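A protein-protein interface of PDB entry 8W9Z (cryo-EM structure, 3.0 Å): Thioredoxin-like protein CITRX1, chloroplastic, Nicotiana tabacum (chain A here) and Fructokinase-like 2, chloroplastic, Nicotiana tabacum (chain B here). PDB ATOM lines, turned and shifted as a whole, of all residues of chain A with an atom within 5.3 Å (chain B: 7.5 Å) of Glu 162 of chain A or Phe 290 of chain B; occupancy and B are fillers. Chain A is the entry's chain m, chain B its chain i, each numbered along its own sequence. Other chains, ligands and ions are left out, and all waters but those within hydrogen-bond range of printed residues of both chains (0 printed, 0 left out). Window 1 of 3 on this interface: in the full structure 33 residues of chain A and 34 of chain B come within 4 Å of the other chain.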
ATOM      1  N   PRO A 103      -3.708   4.217  16.440  1.00  0.00           N
ATOM      2  CA  PRO A 103      -3.580   2.958  15.723  1.00  0.00           C
ATOM      3  C   PRO A 103      -4.916   2.339  15.396  1.00  0.00           C
ATOM      4  O   PRO A 103      -5.068   1.776  14.325  1.00  0.00           O
ATOM      5  CB  PRO A 103      -2.854   2.089  16.715  1.00  0.00           C
ATOM      6  CG  PRO A 103      -1.944   3.031  17.405  1.00  0.00           C
ATOM      7  CD  PRO A 103      -2.732   4.299  17.541  1.00  0.00           C
ATOM      8  N   GLN A 140     -10.602  -9.121  29.823  1.00  0.00           N
ATOM      9  CA  GLN A 140      -9.157  -9.347  29.850  1.00  0.00           C
ATOM     10  C   GLN A 140      -8.479  -8.688  28.648  1.00  0.00           C
ATOM     11  O   GLN A 140      -7.829  -9.336  27.825  1.00  0.00           O
ATOM     12  CB  GLN A 140      -8.832 -10.843  29.924  1.00  0.00           C
ATOM     13  CG  GLN A 140      -9.369 -11.533  31.168  1.00  0.00           C
ATOM     14  CD  GLN A 140      -8.744 -11.008  32.446  1.00  0.00           C
ATOM     15  OE1 GLN A 140      -7.628 -10.488  32.437  1.00  0.00           O
ATOM     16  NE2 GLN A 140      -9.462 -11.142  33.553  1.00  0.00           N
ATOM     17  N   ARG A 142      -5.780  -5.661  27.339  1.00  0.00           N
ATOM     18  CA  ARG A 142      -4.568  -5.000  27.793  1.00  0.00           C
ATOM     19  C   ARG A 142      -4.161  -3.815  26.931  1.00  0.00           C
ATOM     20  O   ARG A 142      -3.228  -3.094  27.305  1.00  0.00           O
ATOM     21  CB  ARG A 142      -3.403  -6.001  27.852  1.00  0.00           C
ATOM     22  CG  ARG A 142      -3.708  -7.249  28.664  1.00  0.00           C
ATOM     23  CD  ARG A 142      -2.479  -8.129  28.827  1.00  0.00           C
ATOM     24  NE  ARG A 142      -1.952  -8.589  27.546  1.00  0.00           N
ATOM     25  CZ  ARG A 142      -0.880  -9.364  27.419  1.00  0.00           C
ATOM     26  NH1 ARG A 142      -0.219  -9.766  28.495  1.00  0.00           N
ATOM     27  NH2 ARG A 142      -0.468  -9.737  26.214  1.00  0.00           N
ATOM     28  N   GLY A 143      -4.829  -3.538  25.832  1.00  0.00           N
ATOM     29  CA  GLY A 143      -4.383  -2.440  25.007  1.00  0.00           C
ATOM     30  C   GLY A 143      -5.448  -2.029  24.052  1.00  0.00           C
ATOM     31  O   GLY A 143      -6.422  -2.729  23.879  1.00  0.00           O
ATOM     32  N   LEU A 144      -5.323  -0.860  23.476  1.00  0.00           N
ATOM     33  CA  LEU A 144      -6.397  -0.428  22.630  1.00  0.00           C
ATOM     34  C   LEU A 144      -6.627  -1.175  21.338  1.00  0.00           C
ATOM     35  O   LEU A 144      -7.760  -1.473  20.998  1.00  0.00           O
ATOM     36  CB  LEU A 144      -6.383   1.066  22.428  1.00  0.00           C
ATOM     37  CG  LEU A 144      -7.436   1.711  23.323  1.00  0.00           C
ATOM     38  CD1 LEU A 144      -8.769   1.069  22.998  1.00  0.00           C
ATOM     39  CD2 LEU A 144      -7.115   1.514  24.796  1.00  0.00           C
ATOM     40  N   PRO A 145      -5.567  -1.503  20.607  1.00  0.00           N
ATOM     41  CA  PRO A 145      -5.929  -2.226  19.386  1.00  0.00           C
ATOM     42  C   PRO A 145      -6.116  -3.729  19.612  1.00  0.00           C
ATOM     43  O   PRO A 145      -5.157  -4.462  19.396  1.00  0.00           O
ATOM     44  CB  PRO A 145      -4.757  -1.944  18.459  1.00  0.00           C
ATOM     45  CG  PRO A 145      -3.616  -1.658  19.359  1.00  0.00           C
ATOM     46  CD  PRO A 145      -4.177  -1.021  20.585  1.00  0.00           C
ATOM     47  N   THR A 146      -7.302  -4.201  20.017  1.00  0.00           N
ATOM     48  CA  THR A 146      -7.462  -5.614  20.324  1.00  0.00           C
ATOM     49  C   THR A 146      -8.675  -6.175  19.597  1.00  0.00           C
ATOM     50  O   THR A 146      -9.668  -5.475  19.377  1.00  0.00           O
ATOM     51  CB  THR A 146      -7.617  -5.854  21.830  1.00  0.00           C
ATOM     52  OG1 THR A 146      -8.697  -5.059  22.334  1.00  0.00           O
ATOM     53  CG2 THR A 146      -6.336  -5.491  22.563  1.00  0.00           C
ATOM     54  N   ARG A 160      -7.568 -13.964  21.090  1.00  0.00           N
ATOM     55  CA  ARG A 160      -7.384 -12.550  21.378  1.00  0.00           C
ATOM     56  C   ARG A 160      -6.113 -12.068  20.723  1.00  0.00           C
ATOM     57  O   ARG A 160      -5.041 -12.629  20.947  1.00  0.00           O
ATOM     58  CB  ARG A 160      -7.298 -12.321  22.884  1.00  0.00           C
ATOM     59  CG  ARG A 160      -7.028 -10.885  23.298  1.00  0.00           C
ATOM     60  CD  ARG A 160      -6.765 -10.797  24.792  1.00  0.00           C
ATOM     61  NE  ARG A 160      -5.475 -11.376  25.158  1.00  0.00           N
ATOM     62  CZ  ARG A 160      -5.052 -11.533  26.409  1.00  0.00           C
ATOM     63  NH1 ARG A 160      -5.815 -11.160  27.424  1.00  0.00           N
ATOM     64  NH2 ARG A 160      -3.860 -12.060  26.645  1.00  0.00           N
ATOM     65  N   THR A 161      -6.222 -11.029  19.908  1.00  0.00           N
ATOM     66  CA  THR A 161      -5.046 -10.475  19.262  1.00  0.00           C
ATOM     67  C   THR A 161      -4.760  -9.110  19.839  1.00  0.00           C
ATOM     68  O   THR A 161      -5.683  -8.352  20.119  1.00  0.00           O
ATOM     69  CB  THR A 161      -5.219 -10.365  17.743  1.00  0.00           C
ATOM     70  OG1 THR A 161      -6.240  -9.409  17.443  1.00  0.00           O
ATOM     71  CG2 THR A 161      -5.597 -11.712  17.158  1.00  0.00           C
ATOM     72  N   GLU A 162      -3.487  -8.795  20.030  1.00  0.00           N
ATOM     73  CA  GLU A 162      -3.104  -7.518  20.629  1.00  0.00           C
ATOM     74  C   GLU A 162      -2.105  -6.831  19.706  1.00  0.00           C
ATOM     75  O   GLU A 162      -0.944  -7.242  19.618  1.00  0.00           O
ATOM     76  CB  GLU A 162      -2.514  -7.718  22.022  1.00  0.00           C
ATOM     77  CG  GLU A 162      -3.439  -8.409  23.008  1.00  0.00           C
ATOM     78  CD  GLU A 162      -2.838  -8.502  24.395  1.00  0.00           C
ATOM     79  OE1 GLU A 162      -1.905  -7.727  24.692  1.00  0.00           O
ATOM     80  OE2 GLU A 162      -3.293  -9.353  25.187  1.00  0.00           O
ATOM     81  N   GLY A 163      -2.554  -5.785  19.017  1.00  0.00           N
ATOM     82  CA  GLY A 163      -1.698  -4.976  18.182  1.00  0.00           C
ATOM     83  C   GLY A 163      -2.287  -4.796  16.806  1.00  0.00           C
ATOM     84  O   GLY A 163      -3.411  -5.222  16.518  1.00  0.00           O
ATOM     85  N   LEU A 164      -1.516  -4.149  15.937  1.00  0.00           N
ATOM     86  CA  LEU A 164      -1.909  -3.928  14.548  1.00  0.00           C
ATOM     87  C   LEU A 164      -1.375  -5.093  13.723  1.00  0.00           C
ATOM     88  O   LEU A 164      -0.202  -5.114  13.342  1.00  0.00           O
ATOM     89  CB  LEU A 164      -1.376  -2.591  14.047  1.00  0.00           C
ATOM     90  CG  LEU A 164      -1.999  -1.990  12.786  1.00  0.00           C
ATOM     91  CD1 LEU A 164      -3.399  -1.475  13.071  1.00  0.00           C
ATOM     92  CD2 LEU A 164      -1.120  -0.881  12.233  1.00  0.00           C
ATOM     93  N   ILE A 165      -2.235  -6.068  13.451  1.00  0.00           N
ATOM     94  CA  ILE A 165      -1.836  -7.276  12.730  1.00  0.00           C
ATOM     95  C   ILE A 165      -2.260  -7.151  11.271  1.00  0.00           C
ATOM     96  O   ILE A 165      -3.250  -6.469  10.972  1.00  0.00           O
ATOM     97  CB  ILE A 165      -2.436  -8.533  13.380  1.00  0.00           C
ATOM     98  CG1 ILE A 165      -3.961  -8.432  13.438  1.00  0.00           C
ATOM     99  CG2 ILE A 165      -1.861  -8.737  14.774  1.00  0.00           C
ATOM    100  CD1 ILE A 165      -4.628  -9.643  14.049  1.00  0.00           C
ATOM    101  N   ALA B 286       7.519  -7.700  21.803  1.00  0.00           N
ATOM    102  CA  ALA B 286       7.723  -7.047  20.515  1.00  0.00           C
ATOM    103  C   ALA B 286       6.382  -6.997  19.797  1.00  0.00           C
ATOM    104  O   ALA B 286       5.916  -8.014  19.271  1.00  0.00           O
ATOM    105  CB  ALA B 286       8.770  -7.783  19.681  1.00  0.00           C
ATOM    106  N   GLN B 287       5.764  -5.820  19.778  1.00  0.00           N
ATOM    107  CA  GLN B 287       4.459  -5.622  19.167  1.00  0.00           C
ATOM    108  C   GLN B 287       4.552  -4.504  18.138  1.00  0.00           C
ATOM    109  O   GLN B 287       5.611  -3.902  17.933  1.00  0.00           O
ATOM    110  CB  GLN B 287       3.399  -5.311  20.230  1.00  0.00           C
ATOM    111  CG  GLN B 287       3.103  -6.476  21.158  1.00  0.00           C
ATOM    112  CD  GLN B 287       2.363  -6.052  22.407  1.00  0.00           C
ATOM    113  OE1 GLN B 287       1.603  -6.827  22.987  1.00  0.00           O
ATOM    114  NE2 GLN B 287       2.587  -4.815  22.833  1.00  0.00           N
ATOM    115  N   HIS B 288       3.429  -4.227  17.483  1.00  0.00           N
ATOM    116  CA  HIS B 288       3.365  -3.214  16.438  1.00  0.00           C
ATOM    117  C   HIS B 288       2.116  -2.376  16.649  1.00  0.00           C
ATOM    118  O   HIS B 288       1.000  -2.899  16.579  1.00  0.00           O
ATOM    119  CB  HIS B 288       3.356  -3.858  15.048  1.00  0.00           C
ATOM    120  CG  HIS B 288       3.311  -2.873  13.924  1.00  0.00           C
ATOM    121  ND1 HIS B 288       4.299  -1.935  13.715  1.00  0.00           N
ATOM    122  CD2 HIS B 288       2.398  -2.680  12.942  1.00  0.00           C
ATOM    123  CE1 HIS B 288       3.996  -1.207  12.656  1.00  0.00           C
ATOM    124  NE2 HIS B 288       2.847  -1.639  12.169  1.00  0.00           N
ATOM    125  N   ALA B 289       2.309  -1.082  16.911  1.00  0.00           N
ATOM    126  CA  ALA B 289       1.218  -0.132  17.114  1.00  0.00           C
ATOM    127  C   ALA B 289       0.301  -0.584  18.252  1.00  0.00           C
ATOM    128  O   ALA B 289      -0.890  -0.848  18.068  1.00  0.00           O
ATOM    129  CB  ALA B 289       0.432   0.085  15.817  1.00  0.00           C
ATOM    130  N   PHE B 290       0.853  -0.706  19.447  1.00  0.00           N
ATOM    131  CA  PHE B 290       0.051  -1.097  20.590  1.00  0.00           C
ATOM    132  C   PHE B 290       0.202  -0.039  21.643  1.00  0.00           C
ATOM    133  O   PHE B 290       1.313   0.286  22.021  1.00  0.00           O
ATOM    134  CB  PHE B 290       0.580  -2.402  21.117  1.00  0.00           C
ATOM    135  CG  PHE B 290      -0.211  -2.984  22.241  1.00  0.00           C
ATOM    136  CD1 PHE B 290      -1.317  -3.763  21.986  1.00  0.00           C
ATOM    137  CD2 PHE B 290       0.184  -2.794  23.549  1.00  0.00           C
ATOM    138  CE1 PHE B 290      -2.034  -4.323  23.016  1.00  0.00           C
ATOM    139  CE2 PHE B 290      -0.528  -3.350  24.585  1.00  0.00           C
ATOM    140  CZ  PHE B 290      -1.633  -4.123  24.316  1.00  0.00           C
ATOM    141  N   VAL B 291      -0.903   0.515  22.114  1.00  0.00           N
ATOM    142  CA  VAL B 291      -0.844   1.552  23.117  1.00  0.00           C
ATOM    143  C   VAL B 291      -1.432   1.033  24.380  1.00  0.00           C
ATOM    144  O   VAL B 291      -2.535   0.524  24.384  1.00  0.00           O
ATOM    145  CB  VAL B 291      -1.615   2.789  22.694  1.00  0.00           C
ATOM    146  N   PRO B 292      -0.693   1.139  25.465  1.00  0.00           N
ATOM    147  CA  PRO B 292      -1.172   0.561  26.707  1.00  0.00           C
ATOM    148  C   PRO B 292      -2.469   1.136  27.173  1.00  0.00           C
ATOM    149  O   PRO B 292      -3.446   0.413  27.248  1.00  0.00           O
ATOM    150  CB  PRO B 292      -0.104   0.968  27.682  1.00  0.00           C
ATOM    151  CG  PRO B 292       1.140   0.991  26.871  1.00  0.00           C
ATOM    152  CD  PRO B 292       0.715   1.549  25.549  1.00  0.00           C
ATOM    153  N   SER B 293      -2.488   2.412  27.497  1.00  0.00           N
ATOM    154  CA  SER B 293      -3.688   3.051  28.024  1.00  0.00           C
ATOM    155  C   SER B 293      -3.691   4.508  27.575  1.00  0.00           C
ATOM    156  O   SER B 293      -2.838   4.937  26.790  1.00  0.00           O
ATOM    157  CB  SER B 293      -3.750   2.921  29.549  1.00  0.00           C
ATOM    158  OG  SER B 293      -2.630   3.538  30.159  1.00  0.00           O
ATOM    159  N   ALA B 322      -1.205   8.858  25.484  1.00  0.00           N
ATOM    160  CA  ALA B 322      -0.789   7.557  25.974  1.00  0.00           C
ATOM    161  C   ALA B 322       0.552   7.671  26.696  1.00  0.00           C
ATOM    162  O   ALA B 322       1.385   8.508  26.342  1.00  0.00           O
ATOM    163  CB  ALA B 322      -0.675   6.564  24.823  1.00  0.00           C
ATOM    164  N   GLY B 324       3.157   5.677  26.666  1.00  0.00           N
ATOM    165  CA  GLY B 324       4.263   5.370  25.785  1.00  0.00           C
ATOM    166  C   GLY B 324       3.859   4.349  24.748  1.00  0.00           C
ATOM    167  O   GLY B 324       2.675   4.078  24.541  1.00  0.00           O
ATOM    168  N   GLY B 325       4.869   3.785  24.092  1.00  0.00           N
ATOM    169  CA  GLY B 325       4.638   2.756  23.099  1.00  0.00           C
ATOM    170  C   GLY B 325       4.946   1.367  23.613  1.00  0.00           C
ATOM    171  O   GLY B 325       4.235   0.844  24.477  1.00  0.00           O
ATOM    172  N   CYS B 326       6.006   0.758  23.090  1.00  0.00           N
ATOM    173  CA  CYS B 326       6.420  -0.574  23.498  1.00  0.00           C
ATOM    174  C   CYS B 326       7.931  -0.587  23.678  1.00  0.00           C
ATOM    175  O   CYS B 326       8.619   0.402  23.407  1.00  0.00           O
ATOM    176  CB  CYS B 326       5.985  -1.634  22.480  1.00  0.00           C
ATOM    177  SG  CYS B 326       6.315  -3.335  22.986  1.00  0.00           S
ATOM    178  N   ASN B 329       9.743  -0.191  20.313  1.00  0.00           N
ATOM    179  CA  ASN B 329       9.797   1.190  19.843  1.00  0.00           C
ATOM    180  C   ASN B 329      10.909   1.965  20.540  1.00  0.00           C
ATOM    181  O   ASN B 329      11.644   2.724  19.897  1.00  0.00           O
ATOM    182  CB  ASN B 329       8.448   1.871  20.062  1.00  0.00           C
ATOM    183  CG  ASN B 329       7.319   1.173  19.332  1.00  0.00           C
ATOM    184  OD1 ASN B 329       7.526   0.569  18.279  1.00  0.00           O
ATOM    185  ND2 ASN B 329       6.116   1.253  19.887  1.00  0.00           N
ATOM    186  N   PHE B 352       4.823 -12.964  10.958  1.00  0.00           N
ATOM    187  CA  PHE B 352       4.761 -11.710  11.703  1.00  0.00           C
ATOM    188  C   PHE B 352       5.970 -11.547  12.618  1.00  0.00           C
ATOM    189  O   PHE B 352       6.573 -10.468  12.675  1.00  0.00           O
ATOM    190  CB  PHE B 352       3.463 -11.644  12.505  1.00  0.00           C
ATOM    191  CG  PHE B 352       3.165 -10.285  13.069  1.00  0.00           C
ATOM    192  CD1 PHE B 352       2.746  -9.257  12.245  1.00  0.00           C
ATOM    193  CD2 PHE B 352       3.294 -10.040  14.424  1.00  0.00           C
ATOM    194  CE1 PHE B 352       2.469  -8.006  12.761  1.00  0.00           C
ATOM    195  CE2 PHE B 352       3.016  -8.792  14.946  1.00  0.00           C
ATOM    196  CZ  PHE B 352       2.605  -7.774  14.113  1.00  0.00           C
ATOM    197  N   THR B 378       2.794 -15.375  17.442  1.00  0.00           N
ATOM    198  CA  THR B 378       3.284 -14.090  17.949  1.00  0.00           C
ATOM    199  C   THR B 378       2.261 -13.334  18.799  1.00  0.00           C
ATOM    200  O   THR B 378       2.495 -13.096  19.980  1.00  0.00           O
ATOM    201  CB  THR B 378       3.781 -13.179  16.811  1.00  0.00           C
ATOM    202  OG1 THR B 378       4.729 -13.891  16.010  1.00  0.00           O
ATOM    203  CG2 THR B 378       4.451 -11.935  17.376  1.00  0.00           C
ATOM    204  N   ALA B 379       1.142 -12.935  18.206  1.00  0.00           N
ATOM    205  CA  ALA B 379       0.142 -12.154  18.939  1.00  0.00           C
ATOM    206  C   ALA B 379      -1.125 -12.916  19.308  1.00  0.00           C
ATOM    207  O   ALA B 379      -2.110 -12.304  19.718  1.00  0.00           O
ATOM    208  CB  ALA B 379      -0.211 -10.895  18.162  1.00  0.00           C
ATOM    209  N   ILE B 380      -1.124 -14.237  19.171  1.00  0.00           N
ATOM    210  CA  ILE B 380      -2.350 -15.001  19.406  1.00  0.00           C
ATOM    211  C   ILE B 380      -2.472 -15.567  20.811  1.00  0.00           C
ATOM    212  O   ILE B 380      -1.593 -16.294  21.269  1.00  0.00           O
ATOM    213  CB  ILE B 380      -2.455 -16.166  18.401  1.00  0.00           C
ATOM    214  CG1 ILE B 380      -2.354 -15.647  16.963  1.00  0.00           C
ATOM    215  CG2 ILE B 380      -3.739 -16.955  18.606  1.00  0.00           C
ATOM    216  CD1 ILE B 380      -3.492 -14.744  16.551  1.00  0.00           C
ATOM    217  N   THR B 381      -3.562 -15.238  21.498  1.00  0.00           N
ATOM    218  CA  THR B 381      -3.800 -15.768  22.833  1.00  0.00           C
ATOM    219  C   THR B 381      -5.130 -16.498  22.823  1.00  0.00           C
ATOM    220  O   THR B 381      -6.123 -15.968  22.340  1.00  0.00           O
ATOM    221  CB  THR B 381      -3.900 -14.644  23.869  1.00  0.00           C
ATOM    222  OG1 THR B 381      -3.004 -13.583  23.519  1.00  0.00           O
ATOM    223  CG2 THR B 381      -3.568 -15.165  25.259  1.00  0.00           C
ATOM    224  N   MET B 383      -8.461 -17.985  24.630  1.00  0.00           N
ATOM    225  CA  MET B 383      -9.247 -17.650  25.817  1.00  0.00           C
ATOM    226  C   MET B 383     -10.478 -18.531  25.986  1.00  0.00           C
ATOM    227  O   MET B 383     -10.958 -19.120  25.020  1.00  0.00           O
ATOM    228  CB  MET B 383      -9.722 -16.196  25.738  1.00  0.00           C
ATOM    229  CG  MET B 383      -8.734 -15.213  25.132  1.00  0.00           C
ATOM    230  SD  MET B 383      -7.474 -14.676  26.300  1.00  0.00           S
ATOM    231  CE  MET B 383      -8.493 -13.857  27.523  1.00  0.00           C
ATOM    232  N   SER B 399       0.783 -16.199  24.890  1.00  0.00           N
ATOM    233  CA  SER B 399       1.358 -15.728  23.632  1.00  0.00           C
ATOM    234  C   SER B 399       2.833 -15.991  23.689  1.00  0.00           C
ATOM    235  O   SER B 399       3.358 -16.307  24.746  1.00  0.00           O
ATOM    236  CB  SER B 399       1.164 -14.240  23.496  1.00  0.00           C
ATOM    237  OG  SER B 399      -0.064 -13.842  24.072  1.00  0.00           O
ATOM    238  N   GLU B 401       4.973 -13.747  23.475  1.00  0.00           N
ATOM    239  CA  GLU B 401       5.499 -12.636  24.237  1.00  0.00           C
ATOM    240  C   GLU B 401       5.460 -12.842  25.720  1.00  0.00           C
ATOM    241  O   GLU B 401       6.396 -12.477  26.414  1.00  0.00           O
ATOM    242  CB  GLU B 401       4.666 -11.414  23.912  1.00  0.00           C
ATOM    243  CG  GLU B 401       4.241 -11.328  22.457  1.00  0.00           C
ATOM    244  CD  GLU B 401       5.421 -11.263  21.510  1.00  0.00           C
ATOM    245  OE1 GLU B 401       6.246 -10.340  21.646  1.00  0.00           O
ATOM    246  OE2 GLU B 401       5.520 -12.138  20.627  1.00  0.00           O
ATOM    247  N   ASP B 402       4.388 -13.423  26.224  1.00  0.00           N
ATOM    248  CA  ASP B 402       4.252 -13.559  27.664  1.00  0.00           C
ATOM    249  C   ASP B 402       4.710 -14.905  28.149  1.00  0.00           C
ATOM    250  O   ASP B 402       4.445 -15.287  29.281  1.00  0.00           O
ATOM    251  CB  ASP B 402       2.842 -13.233  28.143  1.00  0.00           C
ATOM    252  CG  ASP B 402       1.773 -13.899  27.317  1.00  0.00           C
ATOM    253  OD1 ASP B 402       1.760 -15.139  27.263  1.00  0.00           O
ATOM    254  OD2 ASP B 402       0.929 -13.184  26.739  1.00  0.00           O
ATOM    255  N   PHE B 425       4.201  -3.887  31.515  1.00  0.00           N
ATOM    256  CA  PHE B 425       3.328  -4.683  30.661  1.00  0.00           C
ATOM    257  C   PHE B 425       3.675  -6.164  30.729  1.00  0.00           C
ATOM    258  O   PHE B 425       2.786  -7.014  30.604  1.00  0.00           O
ATOM    259  CB  PHE B 425       3.409  -4.181  29.219  1.00  0.00           C
ATOM    260  CG  PHE B 425       2.565  -4.963  28.254  1.00  0.00           C
ATOM    261  CD1 PHE B 425       1.202  -4.744  28.172  1.00  0.00           C
ATOM    262  CD2 PHE B 425       3.139  -5.907  27.420  1.00  0.00           C
ATOM    263  CE1 PHE B 425       0.424  -5.459  27.283  1.00  0.00           C
ATOM    264  CE2 PHE B 425       2.366  -6.625  26.528  1.00  0.00           C
ATOM    265  CZ  PHE B 425       1.008  -6.400  26.460  1.00  0.00           C
ATOM    266  N   LEU B 428       2.275  -8.540  33.876  1.00  0.00           N
ATOM    267  CA  LEU B 428       0.860  -8.869  34.014  1.00  0.00           C
ATOM    268  C   LEU B 428       0.652 -10.374  34.140  1.00  0.00           C
ATOM    269  O   LEU B 428      -0.039 -10.837  35.053  1.00  0.00           O
ATOM    270  CB  LEU B 428       0.075  -8.313  32.826  1.00  0.00           C
ATOM    271  CG  LEU B 428       0.126  -6.794  32.656  1.00  0.00           C
ATOM    272  CD1 LEU B 428      -0.696  -6.358  31.456  1.00  0.00           C
ATOM    273  CD2 LEU B 428      -0.354  -6.101  33.919  1.00  0.00           C
ATOM    274  N   PRO B 457      -1.081  -0.472  32.260  1.00  0.00           N
ATOM    275  CA  PRO B 457      -2.050  -0.876  31.234  1.00  0.00           C
ATOM    276  C   PRO B 457      -3.488  -0.702  31.693  1.00  0.00           C
ATOM    277  O   PRO B 457      -3.744  -0.223  32.802  1.00  0.00           O
ATOM    278  CB  PRO B 457      -1.707  -2.351  30.995  1.00  0.00           C
ATOM    279  CG  PRO B 457      -1.105  -2.801  32.277  1.00  0.00           C
ATOM    280  CD  PRO B 457      -0.348  -1.622  32.816  1.00  0.00           C
ATOM    281  N   ASP B 563      -2.220  10.032  19.579  1.00  0.00           N
ATOM    282  CA  ASP B 563      -2.021   9.392  20.873  1.00  0.00           C
ATOM    283  C   ASP B 563      -0.766   9.889  21.578  1.00  0.00           C
ATOM    284  O   ASP B 563      -0.645   9.709  22.795  1.00  0.00           O
ATOM    285  CB  ASP B 563      -1.958   7.873  20.705  1.00  0.00           C
ATOM    286  CG  ASP B 563      -0.960   7.444  19.649  1.00  0.00           C
ATOM    287  OD1 ASP B 563      -0.390   8.325  18.971  1.00  0.00           O
ATOM    288  OD2 ASP B 563      -0.743   6.223  19.496  1.00  0.00           O
ATOM    289  N   SER B 565       2.586   8.951  21.347  1.00  0.00           N
ATOM    290  CA  SER B 565       3.408   7.859  21.855  1.00  0.00           C
ATOM    291  C   SER B 565       4.871   7.986  21.456  1.00  0.00           C
ATOM    292  O   SER B 565       5.761   7.691  22.266  1.00  0.00           O
ATOM    293  CB  SER B 565       2.862   6.516  21.361  1.00  0.00           C
ATOM    294  OG  SER B 565       1.525   6.322  21.788  1.00  0.00           O
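O of His 288 of chain B is in hydrogen-bond range of N of Leu 164 of chain A (2.9 Å). O of Val 291 of chain B is in hydrogen-bond range of N of Leu 144 of chain A (3.2 Å). N of Arg 160 of chain A lies within hydrogen-bond range of O of Thr 381 of chain B. OD2 of Asp 402 of chain B lies within salt-bridge range of NH2 of Arg 142 of chain A (3.8 Å). O of Ala 379 of chain B lies close to O of Arg 160 of chain A (3.2 Å).
N of Ala 322 of chain B lies within hydrogen-bond range of O of Asp 563 of chain B. The side-chain hydroxyl (OG) of Ser 399 of chain B lies within hydrogen-bond range of the side-chain hydroxyl (OG1) of Thr 381 of chain B (3.0 Å). The side-chain carboxylate of Asp 563 of chain B lies within hydrogen-bond range of the side-chain hydroxyl of Ser 565 of chain B. The backbone carbonyl oxygen (O) of Gln 140 of chain A sits at hydrogen-bond distance from the guanidinium group (NH1) of Arg 160 of chain A (2.7 Å). The guanidinium group (NE) of Arg 142 of chain A is in salt-bridge range of the side-chain carboxylate (OE2) of Glu 162 of chain A (2.8 Å). O of Pro 145 of chain A lies within hydrogen-bond range of N of Gly 163 of chain A, 2.9 Å away.
Among the printed residues, pairs that only touch across the chains: Pro 145 of chain A with Ala 289 of chain B (3.1 Å), Gly 143 of chain A with Phe 290 of chain B (3.3 Å), Pro 103 of chain A with Asp 563 of chain B (3.4 Å), Thr 161 of chain A with Ala 379 of chain B (3.5 Å), Arg 142 of chain A with Pro 292 of chain B (3.5 Å), Arg 142 of chain A with Phe 290 of chain B (3.5 Å), Gly 143 of chain A with Val 291 of chain B (3.5 Å), Glu 162 of chain A with Phe 290 of chain B (3.6 Å), Arg 142 of chain A with Leu 428 of chain B (3.6 Å), Arg 142 of chain A with Phe 425 of chain B (3.6 Å), Glu 162 of chain A with Phe 425 of chain B (3.7 Å), Leu 164 of chain A with Ala 289 of chain B (3.7 Å), Thr 161 of chain A with Ile 380 of chain B (3.7 Å), Gly 143 of chain A with Pro 292 of chain B (3.7 Å), Gly 163 of chain A with His 288 of chain B (3.8 Å), Glu 162 of chain A with Ala 379 of chain B (3.8 Å), Pro 103 of chain A with Ala 289 of chain B (3.8 Å), Gly 163 of chain A with Phe 290 of chain B (3.8 Å), Arg 160 of chain A with Met 383 of chain B (3.8 Å), Gln 140 of chain A with Met 383 of chain B (3.9 Å), Arg 160 of chain A with Ile 380 of chain B (3.9 Å), Pro 145 of chain A with Phe 290 of chain B (3.9 Å), Pro 145 of chain A with Val 291 of chain B (3.9 Å) and Leu 164 of chain A with Phe 352 of chain B (3.9 Å).
Of the printed residues of chain B, Gln 140 of chain A touches Met 383 (3.9 Å). Printed residues of chain B within 4 Å of Glu 162 of chain A: Phe 290, Ala 379 and Phe 425. Of chain A, only Arg 142 (3.5 Å), Gly 143 (3.3 Å), Pro 145 (3.9 Å), Glu 162 (3.6 Å) and Gly 163 (3.8 Å) come within 4 Å of Phe 290 of chain B. Printed residues of chain A within 4 Å of Leu 428 of chain B: Arg 142. The nearest printed residue of chain B that does not touch Glu 162 of chain A is Gln 287 of chain B (4.003 Å). The nearest printed residue of chain B that does not touch Pro 103 of chain A is Phe 290 of chain B (5.1 Å).
Hydrophobic or aromatic side chains of chain B that line the printed part of chain A: His 288, Ala 289, Phe 290, Phe 352, Ile 380, Met 383, Phe 425 and Leu 428. Of the 13 printed residues of chain A, 11 touch a printed residue of chain B. Hydrophobic or aromatic side chains of chain A that line the printed part of chain B: Pro 103, Pro 145 and Leu 164. Along chain A the printed residues that touch a printed residue of chain B span positions 103 to 164. Among the printed residues, Asp or Glu carboxylates within 4 Å of a Lys or Arg side-chain nitrogen of the other chain: Arg 142 of chain A with Asp 402 of chain B (3.8 Å).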
